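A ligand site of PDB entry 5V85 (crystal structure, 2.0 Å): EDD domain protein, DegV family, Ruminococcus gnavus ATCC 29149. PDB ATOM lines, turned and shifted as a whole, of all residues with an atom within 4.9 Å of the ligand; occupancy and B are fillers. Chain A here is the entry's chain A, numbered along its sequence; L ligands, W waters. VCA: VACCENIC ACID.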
ATOM      1  N   CYS A  29      -2.881  -1.777 -17.704  1.00  0.00           N
ATOM      2  CA  CYS A  29      -1.939  -0.667 -17.750  1.00  0.00           C
ATOM      3  C   CYS A  29      -1.594  -0.192 -16.341  1.00  0.00           C
ATOM      4  O   CYS A  29      -0.443   0.213 -16.089  1.00  0.00           O
ATOM      5  CB  CYS A  29      -2.518   0.488 -18.575  1.00  0.00           C
ATOM      6  SG  CYS A  29      -1.368   1.860 -18.797  1.00  0.00           S
ATOM      7  N   LEU A  47      -4.904  -6.032 -21.183  1.00  0.00           N
ATOM      8  CA  LEU A  47      -5.038  -5.559 -22.552  1.00  0.00           C
ATOM      9  C   LEU A  47      -4.258  -6.473 -23.487  1.00  0.00           C
ATOM     10  O   LEU A  47      -3.580  -7.416 -23.060  1.00  0.00           O
ATOM     11  CB  LEU A  47      -4.577  -4.109 -22.671  1.00  0.00           C
ATOM     12  CG  LEU A  47      -5.560  -3.016 -22.276  1.00  0.00           C
ATOM     13  CD1 LEU A  47      -5.507  -2.740 -20.797  1.00  0.00           C
ATOM     14  CD2 LEU A  47      -5.277  -1.759 -23.055  1.00  0.00           C
ATOM     15  N   THR A  80      -1.888  -1.942 -29.753  1.00  0.00           N
ATOM     16  CA  THR A  80      -2.523  -2.470 -28.546  1.00  0.00           C
ATOM     17  C   THR A  80      -4.032  -2.501 -28.739  1.00  0.00           C
ATOM     18  O   THR A  80      -4.576  -1.858 -29.647  1.00  0.00           O
ATOM     19  CB  THR A  80      -2.151  -1.639 -27.302  1.00  0.00           C
ATOM     20  OG1 THR A  80      -2.508  -0.264 -27.519  1.00  0.00           O
ATOM     21  CG2 THR A  80      -0.661  -1.741 -26.999  1.00  0.00           C
ATOM     22  N   SER A  81      -4.707  -3.254 -27.873  1.00  0.00           N
ATOM     23  CA  SER A  81      -6.158  -3.351 -27.907  1.00  0.00           C
ATOM     24  C   SER A  81      -6.702  -3.364 -26.492  1.00  0.00           C
ATOM     25  O   SER A  81      -6.108  -3.984 -25.605  1.00  0.00           O
ATOM     26  CB  SER A  81      -6.622  -4.604 -28.672  1.00  0.00           C
ATOM     27  OG  SER A  81      -6.006  -5.770 -28.150  1.00  0.00           O
ATOM     28  N   CYS A  82      -7.817  -2.677 -26.283  1.00  0.00           N
ATOM     29  CA  CYS A  82      -8.435  -2.647 -24.975  1.00  0.00           C
ATOM     30  C   CYS A  82      -9.133  -3.967 -24.679  1.00  0.00           C
ATOM     31  O   CYS A  82      -9.344  -4.788 -25.585  1.00  0.00           O
ATOM     32  CB  CYS A  82      -9.424  -1.481 -24.899  1.00  0.00           C
ATOM     33  SG  CYS A  82     -10.864  -1.684 -25.975  1.00  0.00           S
ATOM     34  N   LEU A 104      -7.792   3.054 -18.006  1.00  0.00           N
ATOM     35  CA  LEU A 104      -7.092   4.101 -18.739  1.00  0.00           C
ATOM     36  C   LEU A 104      -8.016   5.271 -19.041  1.00  0.00           C
ATOM     37  O   LEU A 104      -9.234   5.094 -19.128  1.00  0.00           O
ATOM     38  CB  LEU A 104      -6.539   3.552 -20.049  1.00  0.00           C
ATOM     39  CG  LEU A 104      -5.237   2.767 -20.001  1.00  0.00           C
ATOM     40  CD1 LEU A 104      -5.251   1.653 -21.026  1.00  0.00           C
ATOM     41  CD2 LEU A 104      -4.083   3.720 -20.243  1.00  0.00           C
ATOM     42  N   SER A 105      -7.426   6.453 -19.226  1.00  0.00           N
ATOM     43  CA  SER A 105      -8.172   7.612 -19.689  1.00  0.00           C
ATOM     44  C   SER A 105      -9.042   7.262 -20.890  1.00  0.00           C
ATOM     45  O   SER A 105      -8.578   6.616 -21.842  1.00  0.00           O
ATOM     46  CB  SER A 105      -7.195   8.737 -20.072  1.00  0.00           C
ATOM     47  OG  SER A 105      -7.889   9.793 -20.723  1.00  0.00           O
ATOM     48  N   LEU A 108      -7.688   8.165 -24.281  1.00  0.00           N
ATOM     49  CA  LEU A 108      -6.534   7.460 -24.813  1.00  0.00           C
ATOM     50  C   LEU A 108      -6.801   6.012 -25.162  1.00  0.00           C
ATOM     51  O   LEU A 108      -5.953   5.376 -25.796  1.00  0.00           O
ATOM     52  CB  LEU A 108      -5.365   7.510 -23.810  1.00  0.00           C
ATOM     53  CG  LEU A 108      -4.918   8.894 -23.325  1.00  0.00           C
ATOM     54  CD1 LEU A 108      -3.873   8.774 -22.221  1.00  0.00           C
ATOM     55  CD2 LEU A 108      -4.386   9.730 -24.482  1.00  0.00           C
ATOM     56  N   SER A 109      -7.948   5.453 -24.783  1.00  0.00           N
ATOM     57  CA  SER A 109      -8.181   4.031 -24.934  1.00  0.00           C
ATOM     58  C   SER A 109      -9.681   3.758 -24.861  1.00  0.00           C
ATOM     59  O   SER A 109     -10.422   4.503 -24.218  1.00  0.00           O
ATOM     60  CB  SER A 109      -7.443   3.227 -23.861  1.00  0.00           C
ATOM     61  OG  SER A 109      -7.811   1.852 -23.883  1.00  0.00           O
ATOM     62  N   GLY A 110     -10.102   2.679 -25.516  1.00  0.00           N
ATOM     63  CA  GLY A 110     -11.466   2.218 -25.414  1.00  0.00           C
ATOM     64  C   GLY A 110     -11.761   1.399 -24.174  1.00  0.00           C
ATOM     65  O   GLY A 110     -12.863   0.854 -24.049  1.00  0.00           O
ATOM     66  N   ARG A 137      -8.714   9.218 -16.304  1.00  0.00           N
ATOM     67  CA  ARG A 137      -8.167  10.374 -17.005  1.00  0.00           C
ATOM     68  C   ARG A 137      -6.641  10.387 -16.934  1.00  0.00           C
ATOM     69  O   ARG A 137      -6.008  11.445 -16.945  1.00  0.00           O
ATOM     70  CB  ARG A 137      -8.764  11.683 -16.470  1.00  0.00           C
ATOM     71  CG  ARG A 137     -10.241  11.866 -16.800  1.00  0.00           C
ATOM     72  CD  ARG A 137     -11.057  12.221 -15.561  1.00  0.00           C
ATOM     73  NE  ARG A 137     -12.488  12.278 -15.849  1.00  0.00           N
ATOM     74  CZ  ARG A 137     -13.406  11.524 -15.269  1.00  0.00           C
ATOM     75  NH1 ARG A 137     -13.062  10.648 -14.331  1.00  0.00           N
ATOM     76  NH2 ARG A 137     -14.687  11.645 -15.599  1.00  0.00           N
ATOM     77  N   SER A 138      -6.053   9.194 -16.870  1.00  0.00           N
ATOM     78  CA  SER A 138      -4.625   9.065 -16.679  1.00  0.00           C
ATOM     79  C   SER A 138      -4.181   7.704 -17.215  1.00  0.00           C
ATOM     80  O   SER A 138      -4.836   7.135 -18.100  1.00  0.00           O
ATOM     81  CB  SER A 138      -4.263   9.223 -15.190  1.00  0.00           C
ATOM     82  OG  SER A 138      -2.905   8.924 -14.940  1.00  0.00           O
ATOM     83  N   ALA A 139      -3.090   7.182 -16.686  1.00  0.00           N
ATOM     84  CA  ALA A 139      -2.558   5.888 -17.125  1.00  0.00           C
ATOM     85  C   ALA A 139      -1.552   5.425 -16.078  1.00  0.00           C
ATOM     86  O   ALA A 139      -1.178   6.177 -15.179  1.00  0.00           O
ATOM     87  CB  ALA A 139      -1.893   6.000 -18.501  1.00  0.00           C
ATOM     88  N   SER A 140      -1.143   4.162 -16.207  1.00  0.00           N
ATOM     89  CA  SER A 140      -0.026   3.594 -15.455  1.00  0.00           C
ATOM     90  C   SER A 140      -0.293   3.807 -13.958  1.00  0.00           C
ATOM     91  O   SER A 140      -1.365   3.435 -13.481  1.00  0.00           O
ATOM     92  CB  SER A 140       1.272   4.188 -15.981  1.00  0.00           C
ATOM     93  OG  SER A 140       2.371   3.875 -15.139  1.00  0.00           O
ATOM     94  N   THR A 176      -0.902  13.969 -13.794  1.00  0.00           N
ATOM     95  CA  THR A 176       0.057  13.027 -14.362  1.00  0.00           C
ATOM     96  C   THR A 176       1.106  13.770 -15.182  1.00  0.00           C
ATOM     97  O   THR A 176       0.779  14.738 -15.880  1.00  0.00           O
ATOM     98  CB  THR A 176      -0.652  11.991 -15.260  1.00  0.00           C
ATOM     99  OG1 THR A 176      -1.679  11.335 -14.504  1.00  0.00           O
ATOM    100  CG2 THR A 176       0.329  10.941 -15.779  1.00  0.00           C
ATOM    101  N   PHE A 178       5.064  12.991 -17.410  1.00  0.00           N
ATOM    102  CA  PHE A 178       6.022  11.999 -17.842  1.00  0.00           C
ATOM    103  C   PHE A 178       7.037  12.605 -18.792  1.00  0.00           C
ATOM    104  O   PHE A 178       6.765  13.606 -19.472  1.00  0.00           O
ATOM    105  CB  PHE A 178       5.345  10.776 -18.490  1.00  0.00           C
ATOM    106  CG  PHE A 178       4.505  11.095 -19.707  1.00  0.00           C
ATOM    107  CD1 PHE A 178       3.206  11.545 -19.581  1.00  0.00           C
ATOM    108  CD2 PHE A 178       5.012  10.886 -20.982  1.00  0.00           C
ATOM    109  CE1 PHE A 178       2.431  11.811 -20.697  1.00  0.00           C
ATOM    110  CE2 PHE A 178       4.241  11.146 -22.109  1.00  0.00           C
ATOM    111  CZ  PHE A 178       2.946  11.611 -21.965  1.00  0.00           C
ATOM    112  N   LEU A 186       3.478   6.619 -28.860  1.00  0.00           N
ATOM    113  CA  LEU A 186       2.307   7.444 -28.574  1.00  0.00           C
ATOM    114  C   LEU A 186       1.914   8.286 -29.790  1.00  0.00           C
ATOM    115  O   LEU A 186       0.729   8.481 -30.058  1.00  0.00           O
ATOM    116  CB  LEU A 186       2.576   8.339 -27.367  1.00  0.00           C
ATOM    117  CG  LEU A 186       2.516   7.698 -25.979  1.00  0.00           C
ATOM    118  CD1 LEU A 186       3.235   8.563 -24.954  1.00  0.00           C
ATOM    119  CD2 LEU A 186       1.080   7.438 -25.556  1.00  0.00           C
ATOM    120  N   ARG A 191      -2.081   9.136 -30.124  1.00  0.00           N
ATOM    121  CA  ARG A 191      -2.326   9.563 -28.750  1.00  0.00           C
ATOM    122  C   ARG A 191      -1.745  10.934 -28.441  1.00  0.00           C
ATOM    123  O   ARG A 191      -1.840  11.391 -27.297  1.00  0.00           O
ATOM    124  CB  ARG A 191      -1.757   8.531 -27.777  1.00  0.00           C
ATOM    125  CG  ARG A 191      -2.758   7.471 -27.329  1.00  0.00           C
ATOM    126  CD  ARG A 191      -3.122   6.519 -28.452  1.00  0.00           C
ATOM    127  NE  ARG A 191      -4.165   5.577 -28.059  1.00  0.00           N
ATOM    128  CZ  ARG A 191      -4.571   4.547 -28.790  1.00  0.00           C
ATOM    129  NH1 ARG A 191      -4.027   4.321 -29.979  1.00  0.00           N
ATOM    130  NH2 ARG A 191      -5.524   3.742 -28.341  1.00  0.00           N
ATOM    131  N   SER A 211      -0.811  15.176 -18.234  1.00  0.00           N
ATOM    132  CA  SER A 211      -2.238  15.085 -18.481  1.00  0.00           C
ATOM    133  C   SER A 211      -2.871  16.472 -18.534  1.00  0.00           C
ATOM    134  O   SER A 211      -2.329  17.452 -18.007  1.00  0.00           O
ATOM    135  CB  SER A 211      -2.923  14.257 -17.397  1.00  0.00           C
ATOM    136  OG  SER A 211      -2.737  14.859 -16.119  1.00  0.00           O
ATOM    137  N   GLY A 215      -8.085  14.293 -19.523  1.00  0.00           N
ATOM    138  CA  GLY A 215      -7.457  13.009 -19.772  1.00  0.00           C
ATOM    139  C   GLY A 215      -6.733  12.883 -21.084  1.00  0.00           C
ATOM    140  O   GLY A 215      -6.456  11.762 -21.528  1.00  0.00           O
ATOM    141  N   THR A 216      -6.425  13.994 -21.746  1.00  0.00           N
ATOM    142  CA  THR A 216      -5.561  13.992 -22.922  1.00  0.00           C
ATOM    143  C   THR A 216      -4.134  14.332 -22.504  1.00  0.00           C
ATOM    144  O   THR A 216      -3.863  14.696 -21.354  1.00  0.00           O
ATOM    145  CB  THR A 216      -6.060  14.982 -23.990  1.00  0.00           C
ATOM    146  OG1 THR A 216      -6.085  16.304 -23.441  1.00  0.00           O
ATOM    147  CG2 THR A 216      -7.462  14.608 -24.456  1.00  0.00           C
ATOM    148  N   ILE A 217      -3.218  14.217 -23.459  1.00  0.00           N
ATOM    149  CA  ILE A 217      -1.805  14.499 -23.222  1.00  0.00           C
ATOM    150  C   ILE A 217      -1.486  15.879 -23.774  1.00  0.00           C
ATOM    151  O   ILE A 217      -1.941  16.247 -24.870  1.00  0.00           O
ATOM    152  CB  ILE A 217      -0.914  13.423 -23.865  1.00  0.00           C
ATOM    153  CG1 ILE A 217      -1.226  12.048 -23.252  1.00  0.00           C
ATOM    154  CG2 ILE A 217       0.548  13.769 -23.708  1.00  0.00           C
ATOM    155  CD1 ILE A 217      -0.539  10.892 -23.959  1.00  0.00           C
ATOM    156  N   ILE A 284       1.474  -2.584 -21.074  1.00  0.00           N
ATOM    157  CA  ILE A 284       0.946  -1.452 -21.839  1.00  0.00           C
ATOM    158  C   ILE A 284       1.778  -0.207 -21.573  1.00  0.00           C
ATOM    159  O   ILE A 284       2.132   0.528 -22.501  1.00  0.00           O
ATOM    160  CB  ILE A 284      -0.544  -1.230 -21.515  1.00  0.00           C
ATOM    161  CG1 ILE A 284      -1.380  -2.405 -22.036  1.00  0.00           C
ATOM    162  CG2 ILE A 284      -1.016   0.090 -22.112  1.00  0.00           C
ATOM    163  CD1 ILE A 284      -1.350  -2.573 -23.550  1.00  0.00           C
ATOM    164  N   SER A 285       2.122   0.042 -20.305  1.00  0.00           N
ATOM    165  CA  SER A 285       2.946   1.202 -19.981  1.00  0.00           C
ATOM    166  C   SER A 285       4.307   1.128 -20.665  1.00  0.00           C
ATOM    167  O   SER A 285       4.815   2.129 -21.180  1.00  0.00           O
ATOM    168  CB  SER A 285       3.109   1.322 -18.468  1.00  0.00           C
ATOM    169  OG  SER A 285       1.871   1.641 -17.852  1.00  0.00           O
ATOM    170  N   TYR A 288       4.106   2.062 -24.498  1.00  0.00           N
ATOM    171  CA  TYR A 288       3.957   3.485 -24.830  1.00  0.00           C
ATOM    172  C   TYR A 288       5.003   4.378 -24.176  1.00  0.00           C
ATOM    173  O   TYR A 288       5.354   5.409 -24.745  1.00  0.00           O
ATOM    174  CB  TYR A 288       2.542   3.954 -24.481  1.00  0.00           C
ATOM    175  CG  TYR A 288       1.524   3.407 -25.461  1.00  0.00           C
ATOM    176  CD1 TYR A 288       1.372   3.971 -26.717  1.00  0.00           C
ATOM    177  CD2 TYR A 288       0.767   2.279 -25.148  1.00  0.00           C
ATOM    178  CE1 TYR A 288       0.471   3.459 -27.638  1.00  0.00           C
ATOM    179  CE2 TYR A 288      -0.136   1.760 -26.056  1.00  0.00           C
ATOM    180  CZ  TYR A 288      -0.286   2.353 -27.295  1.00  0.00           C
ATOM    181  OH  TYR A 288      -1.181   1.829 -28.205  1.00  0.00           O
ATOM    182  N   ALA A 289       5.533   4.000 -23.009  1.00  0.00           N
ATOM    183  CA  ALA A 289       6.600   4.800 -22.403  1.00  0.00           C
ATOM    184  C   ALA A 289       7.956   4.505 -23.022  1.00  0.00           C
ATOM    185  O   ALA A 289       8.801   5.391 -23.099  1.00  0.00           O
ATOM    186  CB  ALA A 289       6.661   4.575 -20.892  1.00  0.00           C
ATOM    187  N   ILE A 295       7.282   8.079 -15.474  1.00  0.00           N
ATOM    188  CA  ILE A 295       5.936   8.625 -15.269  1.00  0.00           C
ATOM    189  C   ILE A 295       5.790   8.977 -13.792  1.00  0.00           C
ATOM    190  O   ILE A 295       6.155   8.172 -12.925  1.00  0.00           O
ATOM    191  CB  ILE A 295       4.849   7.629 -15.700  1.00  0.00           C
ATOM    192  CG1 ILE A 295       5.024   7.247 -17.174  1.00  0.00           C
ATOM    193  CG2 ILE A 295       3.460   8.206 -15.451  1.00  0.00           C
ATOM    194  CD1 ILE A 295       4.437   5.901 -17.527  1.00  0.00           C
HETATM  195  O2  VCA L   1      -6.575   0.872 -25.825  1.00  0.00           O
HETATM  196  C1  VCA L   1      -5.365   0.615 -26.052  1.00  0.00           C
HETATM  197  O1  VCA L   1      -5.045  -0.022 -27.093  1.00  0.00           O
HETATM  198  C2  VCA L   1      -4.277   1.067 -25.074  1.00  0.00           C
HETATM  199  C3  VCA L   1      -3.790   2.470 -25.444  1.00  0.00           C
HETATM  200  C4  VCA L   1      -3.100   3.110 -24.238  1.00  0.00           C
HETATM  201  C5  VCA L   1      -2.424   4.425 -24.654  1.00  0.00           C
HETATM  202  C6  VCA L   1      -1.895   5.164 -23.424  1.00  0.00           C
HETATM  203  C7  VCA L   1      -0.878   4.308 -22.682  1.00  0.00           C
HETATM  204  C8  VCA L   1      -0.066   5.188 -21.726  1.00  0.00           C
HETATM  205  C9  VCA L   1       0.955   4.333 -20.975  1.00  0.00           C
HETATM  206  C10 VCA L   1       1.804   5.197 -20.029  1.00  0.00           C
HETATM  207  C11 VCA L   1       2.758   6.082 -20.833  1.00  0.00           C
HETATM  208  C12 VCA L   1       2.824   7.394 -20.627  1.00  0.00           C
HETATM  209  C13 VCA L   1       1.969   8.091 -19.570  1.00  0.00           C
HETATM  210  C14 VCA L   1       0.694   8.648 -20.220  1.00  0.00           C
HETATM  211  C15 VCA L   1      -0.025   9.577 -19.244  1.00  0.00           C
HETATM  212  C16 VCA L   1      -1.428   9.885 -19.780  1.00  0.00           C
HETATM  213  C17 VCA L   1      -2.064  11.034 -19.004  1.00  0.00           C
HETATM  214  C18 VCA L   1      -3.434  11.374 -19.600  1.00  0.00           C
HETATM  215  O   HOH W   1      -8.634   1.186 -27.506  1.00  0.00           O
HETATM  216  O   HOH W   2      -5.544   0.904 -29.409  1.00  0.00           O
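Water W2 lies within hydrogen-bond range of an oxygen (O1) of the ligand (2.5 Å), the backbone carbonyl oxygen of Thr 80 (2.9 Å) and the guanidinium group of Arg 191 (3.0 Å). Water W1 lies within hydrogen-bond range of O2 of the ligand (2.7 Å) and N of Gly 110 (2.9 Å).
Leu 47 touches the ligand. N of Cys 82 touches O2 of the ligand, at 3.8 Å. Leu 108 touches the ligand. N of Gly 110 touches O2 of the ligand, at 3.97 Å. Arg 137 touches the ligand (O to C18, 3.7 Å). Ser 138 touches the ligand (CA to C18, 3.9 Å). Ala 139 touches the ligand. CG2 of Thr 176 touches C15 of the ligand (3.7 Å). CE1 of Phe 178 touches C15 of the ligand (3.6 Å). Ser 211 touches the ligand. O of Gly 215 touches C18 of the ligand, at 3.6 Å. Thr 216 touches the ligand. Ser 285 touches the ligand. Tyr 288 touches the ligand (CD2 to C7, 3.6 Å). Ile 295 touches the ligand (CD1 to C10, 3.7 Å). 19 residues have an atom within 4 Å of the ligand: Leu 47, Thr 80, Ser 81, Cys 82, Leu 108, Ser 109, Gly 110, Arg 137, Ser 138, Ala 139, Thr 176, Phe 178, Arg 191, Ser 211, Gly 215, Thr 216, Ser 285, Tyr 288 and Ile 295. Along chain A the residues within 4 Å of the ligand span positions 47 to 295. The nearest printed residue that does not touch the ligand is Cys 29 (4.03 Å).
OG of Ser 105 is in hydrogen-bond range of O of Gly 215, at 2.6 Å. The guanidinium group (NE) of Arg 191 sits at hydrogen-bond distance from the backbone carbonyl oxygen (O) of Leu 108, 2.9 Å away. The backbone NH (N) of Arg 191 sits at hydrogen-bond distance from the backbone carbonyl oxygen (O) of Leu 186, at 2.9 Å. The backbone carbonyl oxygen of Thr 176 is in hydrogen-bond range of the backbone NH of Ser 211. OG of Ser 138 lies within hydrogen-bond range of OG1 of Thr 176 (2.7 Å). SG of Cys 82 sits close to O of Gly 110 (3.8 Å). OG of Ser 285 lies within hydrogen-bond range of O of Cys 29, at 3.2 Å. The backbone carbonyl oxygen of Ser 138 sits at hydrogen-bond distance from the backbone NH of Ser 105, at 2.9 Å.
The side-chain hydroxyl (OG) of Ser 109 is in hydrogen-bond range of an oxygen (O2) of the ligand (2.5 Å). O1 of the ligand is in hydrogen-bond range of OG1 of Thr 80 (2.6 Å). N of Ser 81 lies within hydrogen-bond range of O1 of the ligand (3.3 Å). The guanidinium group (NH2) of Arg 191 lies within salt-bridge range of an oxygen (O2) of the ligand (3.96 Å).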
